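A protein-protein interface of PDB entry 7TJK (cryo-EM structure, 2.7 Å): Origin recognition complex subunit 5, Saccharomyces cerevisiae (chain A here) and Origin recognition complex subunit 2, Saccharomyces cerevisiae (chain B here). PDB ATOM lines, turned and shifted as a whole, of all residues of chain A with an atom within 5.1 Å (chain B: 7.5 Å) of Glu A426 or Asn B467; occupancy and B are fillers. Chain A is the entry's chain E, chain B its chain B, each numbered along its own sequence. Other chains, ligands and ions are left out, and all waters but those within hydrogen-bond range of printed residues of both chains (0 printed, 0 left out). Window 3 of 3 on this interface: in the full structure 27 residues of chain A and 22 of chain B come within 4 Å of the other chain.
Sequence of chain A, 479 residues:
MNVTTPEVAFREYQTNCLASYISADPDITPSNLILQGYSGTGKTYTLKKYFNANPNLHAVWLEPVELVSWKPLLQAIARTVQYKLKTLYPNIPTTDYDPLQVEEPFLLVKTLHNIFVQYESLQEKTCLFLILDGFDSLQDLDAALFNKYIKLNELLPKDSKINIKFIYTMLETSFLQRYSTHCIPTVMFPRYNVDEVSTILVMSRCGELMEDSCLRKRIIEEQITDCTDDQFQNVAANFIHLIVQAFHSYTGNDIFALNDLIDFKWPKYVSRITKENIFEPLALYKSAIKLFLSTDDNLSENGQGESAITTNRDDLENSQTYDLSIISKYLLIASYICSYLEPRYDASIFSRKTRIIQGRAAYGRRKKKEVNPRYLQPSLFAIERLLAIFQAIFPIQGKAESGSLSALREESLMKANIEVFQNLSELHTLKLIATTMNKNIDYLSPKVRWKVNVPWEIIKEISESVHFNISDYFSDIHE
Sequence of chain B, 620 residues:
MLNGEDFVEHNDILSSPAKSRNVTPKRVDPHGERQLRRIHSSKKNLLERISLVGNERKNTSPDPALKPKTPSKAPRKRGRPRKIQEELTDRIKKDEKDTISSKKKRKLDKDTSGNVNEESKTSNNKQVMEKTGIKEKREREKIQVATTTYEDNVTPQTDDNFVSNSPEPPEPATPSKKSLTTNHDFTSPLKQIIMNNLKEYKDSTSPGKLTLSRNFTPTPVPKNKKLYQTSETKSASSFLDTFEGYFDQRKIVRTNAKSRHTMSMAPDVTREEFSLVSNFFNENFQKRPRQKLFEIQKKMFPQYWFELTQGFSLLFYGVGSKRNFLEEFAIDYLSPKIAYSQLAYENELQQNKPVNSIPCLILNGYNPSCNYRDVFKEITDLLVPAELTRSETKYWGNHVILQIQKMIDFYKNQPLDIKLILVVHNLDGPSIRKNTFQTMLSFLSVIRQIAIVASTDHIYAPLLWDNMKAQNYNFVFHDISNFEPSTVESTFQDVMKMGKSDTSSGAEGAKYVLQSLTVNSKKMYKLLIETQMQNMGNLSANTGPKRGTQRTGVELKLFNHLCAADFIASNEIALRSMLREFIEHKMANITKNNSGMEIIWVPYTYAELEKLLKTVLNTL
Of the 10 printed residues of chain A, 6 touch a printed residue of chain B.
Hydrophobic or aromatic side chains of chain B within 4 Å of the printed part of chain A: Leu B463 and Ala B470.
Among the printed residues, 12 pairs touch across the chains.
Phe A421 touches Leu B463 (CB to N, 3.7 Å).
Trp B465 touches Gln A422.
O of Asp B466 touches CG of Gln A422 (3.9 Å).
Asn B467 touches Gln A422 (OD1 to CG, 3.3 Å).
Gln A422 touches Ala B470.
Leu B463 touches Leu A424.
N of Asp B466 touches CB of Ser A425, at 3.8 Å.
Glu A426 touches Asp B466.
The backbone NH of Met B468 is in hydrogen-bond range of the side-chain carboxylate of Asp B466, at 2.9 Å.
OD1 of Asp B466 sits at hydrogen-bond distance from N of Lys B469, 2.9 Å away.
O of Phe A421 sits at hydrogen-bond distance from OG of Ser A425 (2.7 Å).
OG1 of Thr A429 is in hydrogen-bond range of O of Ser A425 (2.8 Å).
Glu A426 touches just these residues of chain B: Asp B466 and Asn B467.
Of chain A, only Gln A422 and Glu A426 come within 4 Å of Asn B467.
Printed residues of chain A within 4 Å of Asp B466: Gln A422 (3.9 Å), Ser A425 (3.8 Å), Glu A426 (3.5 Å) and Thr A429 (2.9 Å).
Of the printed residues of chain B, Thr A429 touches Asp B466.
Tyr B473 touches none of the printed residues of chain A.
Lys B469 touches none of the printed residues of chain A.
O of Leu B463 sits at hydrogen-bond distance from OG of Ser A425, at 2.5 Å.
The side-chain hydroxyl (OG) of Ser A425 sits close to the backbone carbonyl oxygen (O) of Trp B465 (3.4 Å).
OG1 of Thr A429 sits at hydrogen-bond distance from OD2 of Asp B466 (2.9 Å).
The backbone NH of Asn B467 lies within hydrogen-bond range of the side-chain carboxylate of Glu A426.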
ATOM      1  N   PHE A 421       2.076  11.828 -16.296  1.00  0.00           N
ATOM      2  CA  PHE A 421       2.269  11.431 -17.687  1.00  0.00           C
ATOM      3  C   PHE A 421       0.956  11.407 -18.460  1.00  0.00           C
ATOM      4  O   PHE A 421       0.944  11.715 -19.658  1.00  0.00           O
ATOM      5  CB  PHE A 421       2.948  10.066 -17.751  1.00  0.00           C
ATOM      6  CG  PHE A 421       4.401  10.098 -17.398  1.00  0.00           C
ATOM      7  CD1 PHE A 421       5.358  10.357 -18.366  1.00  0.00           C
ATOM      8  CD2 PHE A 421       4.813   9.872 -16.097  1.00  0.00           C
ATOM      9  CE1 PHE A 421       6.701  10.388 -18.040  1.00  0.00           C
ATOM     10  CE2 PHE A 421       6.154   9.900 -15.764  1.00  0.00           C
ATOM     11  CZ  PHE A 421       7.098  10.157 -16.737  1.00  0.00           C
ATOM     12  N   GLN A 422      -0.150  11.054 -17.794  1.00  0.00           N
ATOM     13  CA  GLN A 422      -1.464  11.126 -18.431  1.00  0.00           C
ATOM     14  C   GLN A 422      -1.840  12.565 -18.771  1.00  0.00           C
ATOM     15  O   GLN A 422      -2.368  12.835 -19.857  1.00  0.00           O
ATOM     16  CB  GLN A 422      -2.516  10.492 -17.522  1.00  0.00           C
ATOM     17  CG  GLN A 422      -3.840  10.210 -18.205  1.00  0.00           C
ATOM     18  CD  GLN A 422      -4.841   9.544 -17.283  1.00  0.00           C
ATOM     19  OE1 GLN A 422      -6.049   9.612 -17.507  1.00  0.00           O
ATOM     20  NE2 GLN A 422      -4.343   8.884 -16.245  1.00  0.00           N
ATOM     21  N   ASN A 423      -1.548  13.502 -17.863  1.00  0.00           N
ATOM     22  CA  ASN A 423      -1.806  14.915 -18.122  1.00  0.00           C
ATOM     23  C   ASN A 423      -0.907  15.454 -19.228  1.00  0.00           C
ATOM     24  O   ASN A 423      -1.339  16.290 -20.030  1.00  0.00           O
ATOM     25  CB  ASN A 423      -1.618  15.718 -16.838  1.00  0.00           C
ATOM     26  CG  ASN A 423      -2.846  15.697 -15.955  1.00  0.00           C
ATOM     27  OD1 ASN A 423      -3.907  16.187 -16.337  1.00  0.00           O
ATOM     28  ND2 ASN A 423      -2.708  15.127 -14.765  1.00  0.00           N
ATOM     29  N   LEU A 424       0.343  14.987 -19.288  1.00  0.00           N
ATOM     30  CA  LEU A 424       1.247  15.407 -20.355  1.00  0.00           C
ATOM     31  C   LEU A 424       0.790  14.882 -21.714  1.00  0.00           C
ATOM     32  O   LEU A 424       0.854  15.603 -22.722  1.00  0.00           O
ATOM     33  CB  LEU A 424       2.666  14.940 -20.040  1.00  0.00           C
ATOM     34  CG  LEU A 424       3.799  15.411 -20.951  1.00  0.00           C
ATOM     35  CD1 LEU A 424       3.723  16.908 -21.203  1.00  0.00           C
ATOM     36  CD2 LEU A 424       5.132  15.038 -20.337  1.00  0.00           C
ATOM     37  N   SER A 425       0.321  13.630 -21.756  1.00  0.00           N
ATOM     38  CA  SER A 425      -0.243  13.074 -22.983  1.00  0.00           C
ATOM     39  C   SER A 425      -1.503  13.820 -23.400  1.00  0.00           C
ATOM     40  O   SER A 425      -1.749  14.013 -24.596  1.00  0.00           O
ATOM     41  CB  SER A 425      -0.544  11.590 -22.790  1.00  0.00           C
ATOM     42  OG  SER A 425       0.562  10.915 -22.228  1.00  0.00           O
ATOM     43  N   GLU A 426      -2.311  14.243 -22.422  1.00  0.00           N
ATOM     44  CA  GLU A 426      -3.480  15.063 -22.724  1.00  0.00           C
ATOM     45  C   GLU A 426      -3.081  16.426 -23.276  1.00  0.00           C
ATOM     46  O   GLU A 426      -3.744  16.950 -24.176  1.00  0.00           O
ATOM     47  CB  GLU A 426      -4.346  15.227 -21.475  1.00  0.00           C
ATOM     48  CG  GLU A 426      -5.737  15.787 -21.743  1.00  0.00           C
ATOM     49  CD  GLU A 426      -6.422  15.163 -22.948  1.00  0.00           C
ATOM     50  OE1 GLU A 426      -6.515  13.918 -23.017  1.00  0.00           O
ATOM     51  OE2 GLU A 426      -6.919  15.924 -23.805  1.00  0.00           O
ATOM     52  N   LEU A 427      -2.008  17.014 -22.734  1.00  0.00           N
ATOM     53  CA  LEU A 427      -1.503  18.289 -23.238  1.00  0.00           C
ATOM     54  C   LEU A 427      -1.018  18.164 -24.676  1.00  0.00           C
ATOM     55  O   LEU A 427      -1.220  19.074 -25.489  1.00  0.00           O
ATOM     56  CB  LEU A 427      -0.375  18.800 -22.341  1.00  0.00           C
ATOM     57  CG  LEU A 427      -0.748  19.502 -21.034  1.00  0.00           C
ATOM     58  CD1 LEU A 427       0.503  19.951 -20.296  1.00  0.00           C
ATOM     59  CD2 LEU A 427      -1.669  20.680 -21.291  1.00  0.00           C
ATOM     60  N   HIS A 428      -0.371  17.042 -25.007  1.00  0.00           N
ATOM     61  CA  HIS A 428      -0.013  16.793 -26.402  1.00  0.00           C
ATOM     62  C   HIS A 428      -1.250  16.545 -27.262  1.00  0.00           C
ATOM     63  O   HIS A 428      -1.245  16.877 -28.453  1.00  0.00           O
ATOM     64  CB  HIS A 428       0.976  15.625 -26.498  1.00  0.00           C
ATOM     65  CG  HIS A 428       1.564  15.423 -27.867  1.00  0.00           C
ATOM     66  ND1 HIS A 428       0.823  15.008 -28.954  1.00  0.00           N
ATOM     67  CD2 HIS A 428       2.824  15.605 -28.327  1.00  0.00           C
ATOM     68  CE1 HIS A 428       1.603  14.931 -30.017  1.00  0.00           C
ATOM     69  NE2 HIS A 428       2.822  15.290 -29.664  1.00  0.00           N
ATOM     70  N   THR A 429      -2.303  15.955 -26.692  1.00  0.00           N
ATOM     71  CA  THR A 429      -3.541  15.756 -27.442  1.00  0.00           C
ATOM     72  C   THR A 429      -4.232  17.089 -27.725  1.00  0.00           C
ATOM     73  O   THR A 429      -4.765  17.302 -28.821  1.00  0.00           O
ATOM     74  CB  THR A 429      -4.463  14.806 -26.671  1.00  0.00           C
ATOM     75  OG1 THR A 429      -3.800  13.551 -26.484  1.00  0.00           O
ATOM     76  CG2 THR A 429      -5.762  14.556 -27.422  1.00  0.00           C
ATOM     77  N   LEU A 430      -4.178  18.019 -26.772  1.00  0.00           N
ATOM     78  CA  LEU A 430      -4.796  19.334 -26.909  1.00  0.00           C
ATOM     79  C   LEU A 430      -4.021  20.279 -27.821  1.00  0.00           C
ATOM     80  O   LEU A 430      -4.474  21.417 -28.001  1.00  0.00           O
ATOM     81  CB  LEU A 430      -4.950  19.978 -25.533  1.00  0.00           C
ATOM     82  CG  LEU A 430      -5.961  19.335 -24.583  1.00  0.00           C
ATOM     83  CD1 LEU A 430      -5.671  19.733 -23.146  1.00  0.00           C
ATOM     84  CD2 LEU A 430      -7.372  19.695 -24.978  1.00  0.00           C
ATOM     85  N   LEU B 463       3.282   7.805 -20.634  1.00  0.00           N
ATOM     86  CA  LEU B 463       3.152   8.872 -21.621  1.00  0.00           C
ATOM     87  C   LEU B 463       2.402   8.421 -22.875  1.00  0.00           C
ATOM     88  O   LEU B 463       1.896   9.270 -23.616  1.00  0.00           O
ATOM     89  CB  LEU B 463       4.540   9.406 -21.992  1.00  0.00           C
ATOM     90  CG  LEU B 463       4.706  10.679 -22.826  1.00  0.00           C
ATOM     91  CD1 LEU B 463       4.050  11.854 -22.133  1.00  0.00           C
ATOM     92  CD2 LEU B 463       6.173  10.953 -23.100  1.00  0.00           C
ATOM     93  N   TRP B 465      -0.501   7.145 -23.141  1.00  0.00           N
ATOM     94  CA  TRP B 465      -1.954   7.155 -23.041  1.00  0.00           C
ATOM     95  C   TRP B 465      -2.445   8.484 -22.482  1.00  0.00           C
ATOM     96  O   TRP B 465      -2.023   8.904 -21.400  1.00  0.00           O
ATOM     97  CB  TRP B 465      -2.447   6.000 -22.171  1.00  0.00           C
ATOM     98  CG  TRP B 465      -1.758   4.724 -22.501  1.00  0.00           C
ATOM     99  CD1 TRP B 465      -1.840   4.035 -23.667  1.00  0.00           C
ATOM    100  CD2 TRP B 465      -0.945   3.939 -21.625  1.00  0.00           C
ATOM    101  NE1 TRP B 465      -1.082   2.894 -23.598  1.00  0.00           N
ATOM    102  CE2 TRP B 465      -0.531   2.805 -22.348  1.00  0.00           C
ATOM    103  CE3 TRP B 465      -0.513   4.091 -20.305  1.00  0.00           C
ATOM    104  CZ2 TRP B 465       0.294   1.831 -21.798  1.00  0.00           C
ATOM    105  CZ3 TRP B 465       0.305   3.122 -19.761  1.00  0.00           C
ATOM    106  CH2 TRP B 465       0.705   2.010 -20.508  1.00  0.00           C
ATOM    107  N   ASP B 466      -3.348   9.133 -23.221  1.00  0.00           N
ATOM    108  CA  ASP B 466      -4.080  10.294 -22.733  1.00  0.00           C
ATOM    109  C   ASP B 466      -5.286   9.888 -21.888  1.00  0.00           C
ATOM    110  O   ASP B 466      -5.404   8.722 -21.503  1.00  0.00           O
ATOM    111  CB  ASP B 466      -4.393  11.242 -23.920  1.00  0.00           C
ATOM    112  CG  ASP B 466      -5.637  10.859 -24.783  1.00  0.00           C
ATOM    113  OD1 ASP B 466      -6.367   9.861 -24.592  1.00  0.00           O
ATOM    114  OD2 ASP B 466      -5.887  11.631 -25.731  1.00  0.00           O
ATOM    115  N   ASN B 467      -6.180  10.835 -21.592  1.00  0.00           N
ATOM    116  CA  ASN B 467      -7.305  10.544 -20.705  1.00  0.00           C
ATOM    117  C   ASN B 467      -8.326   9.621 -21.367  1.00  0.00           C
ATOM    118  O   ASN B 467      -8.885   8.735 -20.708  1.00  0.00           O
ATOM    119  CB  ASN B 467      -7.962  11.846 -20.255  1.00  0.00           C
ATOM    120  CG  ASN B 467      -7.095  12.629 -19.293  1.00  0.00           C
ATOM    121  OD1 ASN B 467      -5.869  12.598 -19.381  1.00  0.00           O
ATOM    122  ND2 ASN B 467      -7.727  13.339 -18.366  1.00  0.00           N
ATOM    123  N   MET B 468      -8.568   9.806 -22.668  1.00  0.00           N
ATOM    124  CA  MET B 468      -9.495   8.942 -23.396  1.00  0.00           C
ATOM    125  C   MET B 468      -8.961   7.517 -23.506  1.00  0.00           C
ATOM    126  O   MET B 468      -9.700   6.548 -23.276  1.00  0.00           O
ATOM    127  CB  MET B 468      -9.753   9.522 -24.786  1.00  0.00           C
ATOM    128  CG  MET B 468     -10.803   8.790 -25.605  1.00  0.00           C
ATOM    129  SD  MET B 468     -12.473   9.428 -25.363  1.00  0.00           S
ATOM    130  CE  MET B 468     -13.148   8.227 -24.222  1.00  0.00           C
ATOM    131  N   LYS B 469      -7.675   7.374 -23.838  1.00  0.00           N
ATOM    132  CA  LYS B 469      -7.067   6.055 -23.970  1.00  0.00           C
ATOM    133  C   LYS B 469      -6.948   5.344 -22.628  1.00  0.00           C
ATOM    134  O   LYS B 469      -7.160   4.129 -22.557  1.00  0.00           O
ATOM    135  CB  LYS B 469      -5.694   6.174 -24.634  1.00  0.00           C
ATOM    136  CG  LYS B 469      -5.743   6.356 -26.147  1.00  0.00           C
ATOM    137  CD  LYS B 469      -4.545   5.702 -26.822  1.00  0.00           C
ATOM    138  CE  LYS B 469      -4.451   6.087 -28.291  1.00  0.00           C
ATOM    139  NZ  LYS B 469      -4.208   7.544 -28.476  1.00  0.00           N
ATOM    140  N   ALA B 470      -6.616   6.077 -21.560  1.00  0.00           N
ATOM    141  CA  ALA B 470      -6.560   5.465 -20.236  1.00  0.00           C
ATOM    142  C   ALA B 470      -7.946   5.097 -19.729  1.00  0.00           C
ATOM    143  O   ALA B 470      -8.090   4.121 -18.985  1.00  0.00           O
ATOM    144  CB  ALA B 470      -5.873   6.395 -19.239  1.00  0.00           C
ATOM    145  N   GLN B 471      -8.967   5.869 -20.107  1.00  0.00           N
ATOM    146  CA  GLN B 471     -10.334   5.516 -19.741  1.00  0.00           C
ATOM    147  C   GLN B 471     -10.802   4.267 -20.477  1.00  0.00           C
ATOM    148  O   GLN B 471     -11.491   3.421 -19.894  1.00  0.00           O
ATOM    149  CB  GLN B 471     -11.270   6.687 -20.029  1.00  0.00           C
ATOM    150  CG  GLN B 471     -12.621   6.554 -19.381  1.00  0.00           C
ATOM    151  CD  GLN B 471     -13.654   7.472 -19.993  1.00  0.00           C
ATOM    152  OE1 GLN B 471     -13.964   8.530 -19.445  1.00  0.00           O
ATOM    153  NE2 GLN B 471     -14.201   7.067 -21.130  1.00  0.00           N
ATOM    154  N   ASN B 472     -10.449   4.137 -21.759  1.00  0.00           N
ATOM    155  CA  ASN B 472     -10.868   2.971 -22.534  1.00  0.00           C
ATOM    156  C   ASN B 472     -10.118   1.713 -22.109  1.00  0.00           C
ATOM    157  O   ASN B 472     -10.709   0.628 -22.038  1.00  0.00           O
ATOM    158  CB  ASN B 472     -10.673   3.240 -24.023  1.00  0.00           C
ATOM    159  CG  ASN B 472     -11.731   4.163 -24.591  1.00  0.00           C
ATOM    160  OD1 ASN B 472     -12.570   4.685 -23.859  1.00  0.00           O
ATOM    161  ND2 ASN B 472     -11.694   4.374 -25.901  1.00  0.00           N
ATOM    162  N   TYR B 473      -8.807   1.832 -21.870  1.00  0.00           N
ATOM    163  CA  TYR B 473      -8.026   0.757 -21.257  1.00  0.00           C
ATOM    164  C   TYR B 473      -8.557   0.341 -19.889  1.00  0.00           C
ATOM    165  O   TYR B 473      -8.799  -0.853 -19.671  1.00  0.00           O
ATOM    166  CB  TYR B 473      -6.562   1.181 -21.184  1.00  0.00           C
ATOM    167  CG  TYR B 473      -5.783   0.928 -22.454  1.00  0.00           C
ATOM    168  CD1 TYR B 473      -6.166  -0.078 -23.331  1.00  0.00           C
ATOM    169  CD2 TYR B 473      -4.719   1.738 -22.819  1.00  0.00           C
ATOM    170  CE1 TYR B 473      -5.450  -0.332 -24.481  1.00  0.00           C
ATOM    171  CE2 TYR B 473      -4.016   1.505 -23.981  1.00  0.00           C
ATOM    172  CZ  TYR B 473      -4.387   0.477 -24.811  1.00  0.00           C
ATOM    173  OH  TYR B 473      -3.683   0.254 -25.970  1.00  0.00           O
